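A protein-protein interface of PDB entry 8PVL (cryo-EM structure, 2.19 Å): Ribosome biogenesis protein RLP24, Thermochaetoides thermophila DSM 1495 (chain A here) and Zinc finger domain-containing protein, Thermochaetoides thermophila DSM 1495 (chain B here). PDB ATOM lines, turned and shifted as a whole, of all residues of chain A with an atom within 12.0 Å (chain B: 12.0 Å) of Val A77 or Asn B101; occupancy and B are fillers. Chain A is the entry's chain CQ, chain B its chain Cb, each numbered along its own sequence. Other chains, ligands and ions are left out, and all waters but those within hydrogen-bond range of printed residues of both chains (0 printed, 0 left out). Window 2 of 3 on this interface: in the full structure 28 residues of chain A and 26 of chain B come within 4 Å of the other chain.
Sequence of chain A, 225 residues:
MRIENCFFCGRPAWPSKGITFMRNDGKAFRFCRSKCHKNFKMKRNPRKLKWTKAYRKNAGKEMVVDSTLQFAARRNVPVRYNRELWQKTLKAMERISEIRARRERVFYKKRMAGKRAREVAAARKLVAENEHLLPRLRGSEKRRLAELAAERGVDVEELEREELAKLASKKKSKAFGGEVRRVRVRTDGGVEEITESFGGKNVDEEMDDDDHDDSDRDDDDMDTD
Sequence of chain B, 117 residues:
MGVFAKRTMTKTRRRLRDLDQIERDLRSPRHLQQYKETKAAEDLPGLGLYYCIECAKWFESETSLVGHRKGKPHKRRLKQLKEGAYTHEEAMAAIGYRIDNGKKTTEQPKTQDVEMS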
ATOM      1  N   ARG A   2       7.909  20.072  10.514  1.00  0.00           N
ATOM      2  CA  ARG A   2       8.705  19.316   9.562  1.00  0.00           C
ATOM      3  C   ARG A   2       9.500  18.249  10.296  1.00  0.00           C
ATOM      4  O   ARG A   2       9.728  18.333  11.506  1.00  0.00           O
ATOM      5  CB  ARG A   2       9.646  20.227   8.764  1.00  0.00           C
ATOM      6  CG  ARG A   2      10.798  20.793   9.572  1.00  0.00           C
ATOM      7  CD  ARG A   2      11.823  21.465   8.679  1.00  0.00           C
ATOM      8  NE  ARG A   2      12.595  20.501   7.906  1.00  0.00           N
ATOM      9  CZ  ARG A   2      12.469  20.316   6.599  1.00  0.00           C
ATOM     10  NH1 ARG A   2      11.600  21.009   5.884  1.00  0.00           N
ATOM     11  NH2 ARG A   2      13.236  19.412   5.996  1.00  0.00           N
ATOM     12  N   GLN A  70      17.438  13.187  -5.845  1.00  0.00           N
ATOM     13  CA  GLN A  70      17.533  14.596  -6.194  1.00  0.00           C
ATOM     14  C   GLN A  70      16.228  15.355  -5.989  1.00  0.00           C
ATOM     15  O   GLN A  70      16.197  16.569  -6.205  1.00  0.00           O
ATOM     16  CB  GLN A  70      17.982  14.746  -7.651  1.00  0.00           C
ATOM     17  CG  GLN A  70      19.222  13.947  -7.997  1.00  0.00           C
ATOM     18  CD  GLN A  70      20.398  14.297  -7.110  1.00  0.00           C
ATOM     19  OE1 GLN A  70      20.746  15.467  -6.954  1.00  0.00           O
ATOM     20  NE2 GLN A  70      21.019  13.281  -6.522  1.00  0.00           N
ATOM     21  N   PHE A  71      15.158  14.677  -5.583  1.00  0.00           N
ATOM     22  CA  PHE A  71      13.853  15.311  -5.474  1.00  0.00           C
ATOM     23  C   PHE A  71      13.598  15.955  -4.119  1.00  0.00           C
ATOM     24  O   PHE A  71      12.635  16.718  -3.990  1.00  0.00           O
ATOM     25  CB  PHE A  71      12.748  14.292  -5.761  1.00  0.00           C
ATOM     26  CG  PHE A  71      12.697  13.840  -7.188  1.00  0.00           C
ATOM     27  CD1 PHE A  71      11.945  14.534  -8.121  1.00  0.00           C
ATOM     28  CD2 PHE A  71      13.384  12.708  -7.595  1.00  0.00           C
ATOM     29  CE1 PHE A  71      11.886  14.113  -9.435  1.00  0.00           C
ATOM     30  CE2 PHE A  71      13.331  12.284  -8.908  1.00  0.00           C
ATOM     31  CZ  PHE A  71      12.582  12.987  -9.828  1.00  0.00           C
ATOM     32  N   ALA A  72      14.418  15.672  -3.113  1.00  0.00           N
ATOM     33  CA  ALA A  72      14.236  16.217  -1.774  1.00  0.00           C
ATOM     34  C   ALA A  72      15.385  17.164  -1.465  1.00  0.00           C
ATOM     35  O   ALA A  72      16.552  16.759  -1.490  1.00  0.00           O
ATOM     36  CB  ALA A  72      14.161  15.100  -0.733  1.00  0.00           C
ATOM     37  N   ALA A  73      15.055  18.418  -1.172  1.00  0.00           N
ATOM     38  CA  ALA A  73      16.061  19.409  -0.826  1.00  0.00           C
ATOM     39  C   ALA A  73      15.441  20.460   0.079  1.00  0.00           C
ATOM     40  O   ALA A  73      14.220  20.636   0.116  1.00  0.00           O
ATOM     41  CB  ALA A  73      16.661  20.067  -2.074  1.00  0.00           C
ATOM     42  N   ARG A  74      16.300  21.159   0.816  1.00  0.00           N
ATOM     43  CA  ARG A  74      15.866  22.312   1.596  1.00  0.00           C
ATOM     44  C   ARG A  74      15.586  23.467   0.644  1.00  0.00           C
ATOM     45  O   ARG A  74      16.509  24.017   0.038  1.00  0.00           O
ATOM     46  CB  ARG A  74      16.929  22.688   2.622  1.00  0.00           C
ATOM     47  CG  ARG A  74      16.525  23.817   3.550  1.00  0.00           C
ATOM     48  CD  ARG A  74      17.332  23.785   4.831  1.00  0.00           C
ATOM     49  NE  ARG A  74      17.702  25.122   5.277  1.00  0.00           N
ATOM     50  CZ  ARG A  74      17.056  25.805   6.211  1.00  0.00           C
ATOM     51  NH1 ARG A  74      15.989  25.311   6.815  1.00  0.00           N
ATOM     52  NH2 ARG A  74      17.491  27.016   6.546  1.00  0.00           N
ATOM     53  N   ARG A  75      14.315  23.829   0.502  1.00  0.00           N
ATOM     54  CA  ARG A  75      13.899  24.831  -0.473  1.00  0.00           C
ATOM     55  C   ARG A  75      13.990  26.209   0.169  1.00  0.00           C
ATOM     56  O   ARG A  75      13.155  26.573   1.004  1.00  0.00           O
ATOM     57  CB  ARG A  75      12.486  24.546  -0.971  1.00  0.00           C
ATOM     58  CG  ARG A  75      12.273  23.107  -1.393  1.00  0.00           C
ATOM     59  CD  ARG A  75      13.071  22.759  -2.630  1.00  0.00           C
ATOM     60  NE  ARG A  75      12.841  21.381  -3.042  1.00  0.00           N
ATOM     61  CZ  ARG A  75      13.275  20.855  -4.179  1.00  0.00           C
ATOM     62  NH1 ARG A  75      13.976  21.566  -5.046  1.00  0.00           N
ATOM     63  NH2 ARG A  75      13.000  19.584  -4.452  1.00  0.00           N
ATOM     64  N   ASN A  76      15.006  26.972  -0.218  1.00  0.00           N
ATOM     65  CA  ASN A  76      15.223  28.298   0.337  1.00  0.00           C
ATOM     66  C   ASN A  76      14.495  29.395  -0.427  1.00  0.00           C
ATOM     67  O   ASN A  76      14.420  30.525   0.065  1.00  0.00           O
ATOM     68  CB  ASN A  76      16.720  28.601   0.382  1.00  0.00           C
ATOM     69  CG  ASN A  76      17.406  27.951   1.566  1.00  0.00           C
ATOM     70  OD1 ASN A  76      16.755  27.524   2.518  1.00  0.00           O
ATOM     71  ND2 ASN A  76      18.728  27.883   1.518  1.00  0.00           N
ATOM     72  N   VAL A  77      13.956  29.093  -1.604  1.00  0.00           N
ATOM     73  CA  VAL A  77      13.137  30.021  -2.372  1.00  0.00           C
ATOM     74  C   VAL A  77      11.709  29.482  -2.369  1.00  0.00           C
ATOM     75  O   VAL A  77      11.429  28.473  -3.034  1.00  0.00           O
ATOM     76  CB  VAL A  77      13.665  30.200  -3.802  1.00  0.00           C
ATOM     77  CG1 VAL A  77      12.748  31.114  -4.594  1.00  0.00           C
ATOM     78  CG2 VAL A  77      15.078  30.754  -3.774  1.00  0.00           C
ATOM     79  N   PRO A  78      10.785  30.098  -1.637  1.00  0.00           N
ATOM     80  CA  PRO A  78       9.432  29.544  -1.528  1.00  0.00           C
ATOM     81  C   PRO A  78       8.633  29.701  -2.813  1.00  0.00           C
ATOM     82  O   PRO A  78       8.891  30.568  -3.648  1.00  0.00           O
ATOM     83  CB  PRO A  78       8.809  30.357  -0.389  1.00  0.00           C
ATOM     84  CG  PRO A  78       9.550  31.644  -0.412  1.00  0.00           C
ATOM     85  CD  PRO A  78      10.957  31.300  -0.804  1.00  0.00           C
ATOM     86  N   VAL A  79       7.638  28.831  -2.951  1.00  0.00           N
ATOM     87  CA  VAL A  79       6.729  28.817  -4.089  1.00  0.00           C
ATOM     88  C   VAL A  79       5.343  29.196  -3.586  1.00  0.00           C
ATOM     89  O   VAL A  79       4.928  28.761  -2.505  1.00  0.00           O
ATOM     90  CB  VAL A  79       6.720  27.435  -4.776  1.00  0.00           C
ATOM     91  CG1 VAL A  79       5.788  27.418  -5.978  1.00  0.00           C
ATOM     92  CG2 VAL A  79       8.126  27.042  -5.191  1.00  0.00           C
ATOM     93  N   ARG A  80       4.651  30.043  -4.348  1.00  0.00           N
ATOM     94  CA  ARG A  80       3.272  30.398  -4.037  1.00  0.00           C
ATOM     95  C   ARG A  80       2.390  29.155  -4.048  1.00  0.00           C
ATOM     96  O   ARG A  80       2.545  28.277  -4.901  1.00  0.00           O
ATOM     97  CB  ARG A  80       2.763  31.426  -5.047  1.00  0.00           C
ATOM     98  CG  ARG A  80       1.394  32.002  -4.746  1.00  0.00           C
ATOM     99  CD  ARG A  80       1.084  33.150  -5.689  1.00  0.00           C
ATOM    100  NE  ARG A  80       2.152  34.141  -5.695  1.00  0.00           N
ATOM    101  CZ  ARG A  80       2.218  35.177  -4.871  1.00  0.00           C
ATOM    102  NH1 ARG A  80       1.282  35.400  -3.964  1.00  0.00           N
ATOM    103  NH2 ARG A  80       3.251  36.009  -4.959  1.00  0.00           N
ATOM    104  N   TYR A  81       1.478  29.075  -3.079  1.00  0.00           N
ATOM    105  CA  TYR A  81       0.700  27.860  -2.867  1.00  0.00           C
ATOM    106  C   TYR A  81      -0.227  27.575  -4.042  1.00  0.00           C
ATOM    107  O   TYR A  81      -0.913  28.467  -4.548  1.00  0.00           O
ATOM    108  CB  TYR A  81      -0.120  27.959  -1.581  1.00  0.00           C
ATOM    109  CG  TYR A  81      -1.121  26.833  -1.438  1.00  0.00           C
ATOM    110  CD1 TYR A  81      -0.696  25.523  -1.251  1.00  0.00           C
ATOM    111  CD2 TYR A  81      -2.486  27.075  -1.507  1.00  0.00           C
ATOM    112  CE1 TYR A  81      -1.600  24.489  -1.132  1.00  0.00           C
ATOM    113  CE2 TYR A  81      -3.400  26.045  -1.389  1.00  0.00           C
ATOM    114  CZ  TYR A  81      -2.950  24.755  -1.202  1.00  0.00           C
ATOM    115  OH  TYR A  81      -3.850  23.725  -1.080  1.00  0.00           O
ATOM    116  N   ASN A  82      -0.244  26.313  -4.468  1.00  0.00           N
ATOM    117  CA  ASN A  82      -1.033  25.882  -5.616  1.00  0.00           C
ATOM    118  C   ASN A  82      -1.536  24.475  -5.333  1.00  0.00           C
ATOM    119  O   ASN A  82      -0.730  23.557  -5.143  1.00  0.00           O
ATOM    120  CB  ASN A  82      -0.193  25.926  -6.895  1.00  0.00           C
ATOM    121  CG  ASN A  82      -1.037  25.939  -8.151  1.00  0.00           C
ATOM    122  OD1 ASN A  82      -1.827  25.029  -8.394  1.00  0.00           O
ATOM    123  ND2 ASN A  82      -0.869  26.975  -8.961  1.00  0.00           N
ATOM    124  N   LEU A  85      -0.482  21.736  -7.769  1.00  0.00           N
ATOM    125  CA  LEU A  85       0.940  21.455  -7.601  1.00  0.00           C
ATOM    126  C   LEU A  85       1.189  20.600  -6.366  1.00  0.00           C
ATOM    127  O   LEU A  85       2.001  19.670  -6.404  1.00  0.00           O
ATOM    128  CB  LEU A  85       1.738  22.762  -7.522  1.00  0.00           C
ATOM    129  CG  LEU A  85       3.221  22.669  -7.137  1.00  0.00           C
ATOM    130  CD1 LEU A  85       4.022  21.956  -8.210  1.00  0.00           C
ATOM    131  CD2 LEU A  85       3.820  24.044  -6.874  1.00  0.00           C
ATOM    132  N   TRP A  86       0.483  20.887  -5.269  1.00  0.00           N
ATOM    133  CA  TRP A  86       0.656  20.100  -4.052  1.00  0.00           C
ATOM    134  C   TRP A  86       0.141  18.671  -4.222  1.00  0.00           C
ATOM    135  O   TRP A  86       0.787  17.714  -3.766  1.00  0.00           O
ATOM    136  CB  TRP A  86      -0.038  20.797  -2.883  1.00  0.00           C
ATOM    137  CG  TRP A  86       0.921  21.471  -1.950  1.00  0.00           C
ATOM    138  CD1 TRP A  86       1.260  21.063  -0.696  1.00  0.00           C
ATOM    139  CD2 TRP A  86       1.673  22.665  -2.201  1.00  0.00           C
ATOM    140  NE1 TRP A  86       2.174  21.930  -0.147  1.00  0.00           N
ATOM    141  CE2 TRP A  86       2.443  22.922  -1.051  1.00  0.00           C
ATOM    142  CE3 TRP A  86       1.773  23.539  -3.285  1.00  0.00           C
ATOM    143  CZ2 TRP A  86       3.297  24.016  -0.955  1.00  0.00           C
ATOM    144  CZ3 TRP A  86       2.618  24.626  -3.188  1.00  0.00           C
ATOM    145  CH2 TRP A  86       3.369  24.856  -2.032  1.00  0.00           C
ATOM    146  N   GLU B  89      27.510  19.625   6.698  1.00  0.00           N
ATOM    147  CA  GLU B  89      27.457  19.299   5.275  1.00  0.00           C
ATOM    148  C   GLU B  89      27.642  17.803   5.047  1.00  0.00           C
ATOM    149  O   GLU B  89      26.937  17.202   4.226  1.00  0.00           O
ATOM    150  CB  GLU B  89      28.498  20.092   4.462  1.00  0.00           C
ATOM    151  CG  GLU B  89      28.635  21.653   4.590  1.00  0.00           C
ATOM    152  CD  GLU B  89      28.672  22.244   5.995  1.00  0.00           C
ATOM    153  OE1 GLU B  89      29.413  21.718   6.848  1.00  0.00           O
ATOM    154  OE2 GLU B  89      27.953  23.236   6.240  1.00  0.00           O
ATOM    155  N   MET B  92      24.492  16.116   6.073  1.00  0.00           N
ATOM    156  CA  MET B  92      23.523  16.220   4.988  1.00  0.00           C
ATOM    157  C   MET B  92      23.796  15.188   3.896  1.00  0.00           C
ATOM    158  O   MET B  92      22.875  14.508   3.419  1.00  0.00           O
ATOM    159  CB  MET B  92      23.580  17.637   4.418  1.00  0.00           C
ATOM    160  CG  MET B  92      22.333  18.112   3.727  1.00  0.00           C
ATOM    161  SD  MET B  92      22.235  19.909   3.679  1.00  0.00           S
ATOM    162  CE  MET B  92      21.381  20.242   5.215  1.00  0.00           C
ATOM    163  N   TYR B  97      20.593  14.475   1.527  1.00  0.00           N
ATOM    164  CA  TYR B  97      19.867  15.732   1.505  1.00  0.00           C
ATOM    165  C   TYR B  97      20.747  16.815   0.888  1.00  0.00           C
ATOM    166  O   TYR B  97      21.966  16.667   0.783  1.00  0.00           O
ATOM    167  CB  TYR B  97      19.456  16.105   2.931  1.00  0.00           C
ATOM    168  CG  TYR B  97      18.287  17.047   3.063  1.00  0.00           C
ATOM    169  CD1 TYR B  97      17.146  16.894   2.287  1.00  0.00           C
ATOM    170  CD2 TYR B  97      18.320  18.081   3.988  1.00  0.00           C
ATOM    171  CE1 TYR B  97      16.076  17.755   2.423  1.00  0.00           C
ATOM    172  CE2 TYR B  97      17.260  18.945   4.129  1.00  0.00           C
ATOM    173  CZ  TYR B  97      16.141  18.778   3.347  1.00  0.00           C
ATOM    174  OH  TYR B  97      15.086  19.645   3.495  1.00  0.00           O
ATOM    175  N   ARG B  98      20.117  17.909   0.468  1.00  0.00           N
ATOM    176  CA  ARG B  98      20.857  19.018  -0.120  1.00  0.00           C
ATOM    177  C   ARG B  98      20.093  20.313   0.108  1.00  0.00           C
ATOM    178  O   ARG B  98      18.928  20.312   0.509  1.00  0.00           O
ATOM    179  CB  ARG B  98      21.117  18.799  -1.616  1.00  0.00           C
ATOM    180  CG  ARG B  98      19.950  18.212  -2.385  1.00  0.00           C
ATOM    181  CD  ARG B  98      20.090  18.493  -3.871  1.00  0.00           C
ATOM    182  NE  ARG B  98      18.831  18.332  -4.588  1.00  0.00           N
ATOM    183  CZ  ARG B  98      18.282  19.265  -5.354  1.00  0.00           C
ATOM    184  NH1 ARG B  98      18.850  20.448  -5.517  1.00  0.00           N
ATOM    185  NH2 ARG B  98      17.134  19.003  -5.972  1.00  0.00           N
ATOM    186  N   ILE B  99      20.773  21.428  -0.148  1.00  0.00           N
ATOM    187  CA  ILE B  99      20.206  22.764  -0.004  1.00  0.00           C
ATOM    188  C   ILE B  99      19.996  23.347  -1.393  1.00  0.00           C
ATOM    189  O   ILE B  99      20.933  23.402  -2.198  1.00  0.00           O
ATOM    190  CB  ILE B  99      21.110  23.673   0.846  1.00  0.00           C
ATOM    191  CG1 ILE B  99      21.247  23.115   2.262  1.00  0.00           C
ATOM    192  CG2 ILE B  99      20.570  25.092   0.874  1.00  0.00           C
ATOM    193  CD1 ILE B  99      22.374  23.731   3.054  1.00  0.00           C
ATOM    194  N   ASP B 100      18.768  23.777  -1.673  1.00  0.00           N
ATOM    195  CA  ASP B 100      18.401  24.362  -2.958  1.00  0.00           C
ATOM    196  C   ASP B 100      18.226  25.863  -2.755  1.00  0.00           C
ATOM    197  O   ASP B 100      17.261  26.301  -2.120  1.00  0.00           O
ATOM    198  CB  ASP B 100      17.124  23.718  -3.498  1.00  0.00           C
ATOM    199  CG  ASP B 100      16.602  24.400  -4.750  1.00  0.00           C
ATOM    200  OD1 ASP B 100      17.413  24.932  -5.536  1.00  0.00           O
ATOM    201  OD2 ASP B 100      15.370  24.404  -4.949  1.00  0.00           O
ATOM    202  N   ASN B 101      19.158  26.646  -3.296  1.00  0.00           N
ATOM    203  CA  ASN B 101      19.109  28.099  -3.219  1.00  0.00           C
ATOM    204  C   ASN B 101      18.634  28.733  -4.521  1.00  0.00           C
ATOM    205  O   ASN B 101      18.788  29.944  -4.707  1.00  0.00           O
ATOM    206  CB  ASN B 101      20.479  28.654  -2.831  1.00  0.00           C
ATOM    207  CG  ASN B 101      20.846  28.345  -1.398  1.00  0.00           C
ATOM    208  OD1 ASN B 101      19.975  28.180  -0.545  1.00  0.00           O
ATOM    209  ND2 ASN B 101      22.141  28.264  -1.122  1.00  0.00           N
ATOM    210  N   GLY B 102      18.066  27.941  -5.423  1.00  0.00           N
ATOM    211  CA  GLY B 102      17.605  28.447  -6.701  1.00  0.00           C
ATOM    212  C   GLY B 102      18.611  28.233  -7.815  1.00  0.00           C
ATOM    213  O   GLY B 102      18.294  28.402  -8.991  1.00  0.00           O
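The backbone NH (N) of Gly B102 lies within hydrogen-bond range of the side-chain carboxylate (OD1) of Asp B100, 3.1 Å away.
The backbone carbonyl oxygen (O) of Met B92 sits at hydrogen-bond distance from the backbone NH (N) of Tyr B97 (3.0 Å).
NH2 of Arg A75 sits at hydrogen-bond distance from O of Phe A71 (2.9 Å).
The side-chain amide oxygen of Asn B101 sits at hydrogen-bond distance from the side-chain amide nitrogen of Asn A76 (2.4 Å).
O of Arg A74 lies within hydrogen-bond range of N of Asp B100 (2.8 Å).
O of Gln A70 lies within hydrogen-bond range of NH2 of Arg B98, at 2.6 Å.
OD2 of Asp B100 is in salt-bridge range of NH1 of Arg A75, at 3.2 Å.
N of Asn A76 lies within hydrogen-bond range of O of Asp B100 (3.0 Å).
The side-chain hydroxyl of Tyr B97 lies within hydrogen-bond range of the guanidinium group of Arg A2 (3.1 Å).
The backbone NH (N) of Arg A74 lies within hydrogen-bond range of the backbone carbonyl oxygen (O) of Arg B98 (2.8 Å).
N of Arg A74 is in hydrogen-bond range of OH of Tyr B97 (3.3 Å).
Val A77 touches just one residue of chain B: Asn B101 (3.9 Å).
Asn B101 touches just these residues of chain A: Asn A76 and Val A77.
No residue of chain B comes within 4 Å of Pro A78.
No residue of chain B comes within 4 Å of Val A79.
Of chain A, only Arg A74 and Asn A76 come within 4 Å of Ile B99.
No residue of chain A comes within 4 Å of Gly B102.
Of the printed residues of chain A, Tyr B97 touches Arg A2, Ala A72, Ala A73 and Arg A74.
Of the printed residues of chain B, Arg A75 touches Asp B100 (3.2 Å).
Printed residues of chain B within 4 Å of Ala A73: Tyr B97, Arg B98 and Asp B100.
Of the printed residues of chain B, Gln A70 touches Arg B98.
Printed residues of chain B within 4 Å of Arg A2: Tyr B97 (3.1 Å).
The nearest residue of chain B that does not touch Val A77 is Asp B100 (4.4 Å).
The nearest residue of chain A that does not touch Asn B101 is Arg A74 (5.0 Å).
The nearest printed residue of chain A that does not touch Tyr B97 is Arg A75 (5.2 Å).
Of the 16 printed residues of chain A, 8 touch a printed residue of chain B.
Of the 8 printed residues of chain B, 5 touch a printed residue of chain A.
Printed residues of chain B that touch a printed residue of chain A: Tyr B97, Arg B98, Ile B99, Asp B100 and Asn B101.
Hydrophobic or aromatic side chains of chain B within 4 Å of the printed part of chain A: Tyr B97 and Ile B99.
Among the printed residues, Asp or Glu carboxylates within 4 Å of a Lys or Arg side-chain nitrogen of the other chain: Arg A75 with Asp B100 (3.2 Å).
Among the printed residues, pairs that only touch across the chains: Ala A72 with Tyr B97, Ala A72 with Arg B98, Ala A73 with Tyr B97, Ala A73 with Arg B98, Ala A73 with Asp B100, Arg A74 with Ile B99, Asn A76 with Ile B99 and Val A77 with Asn B101.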
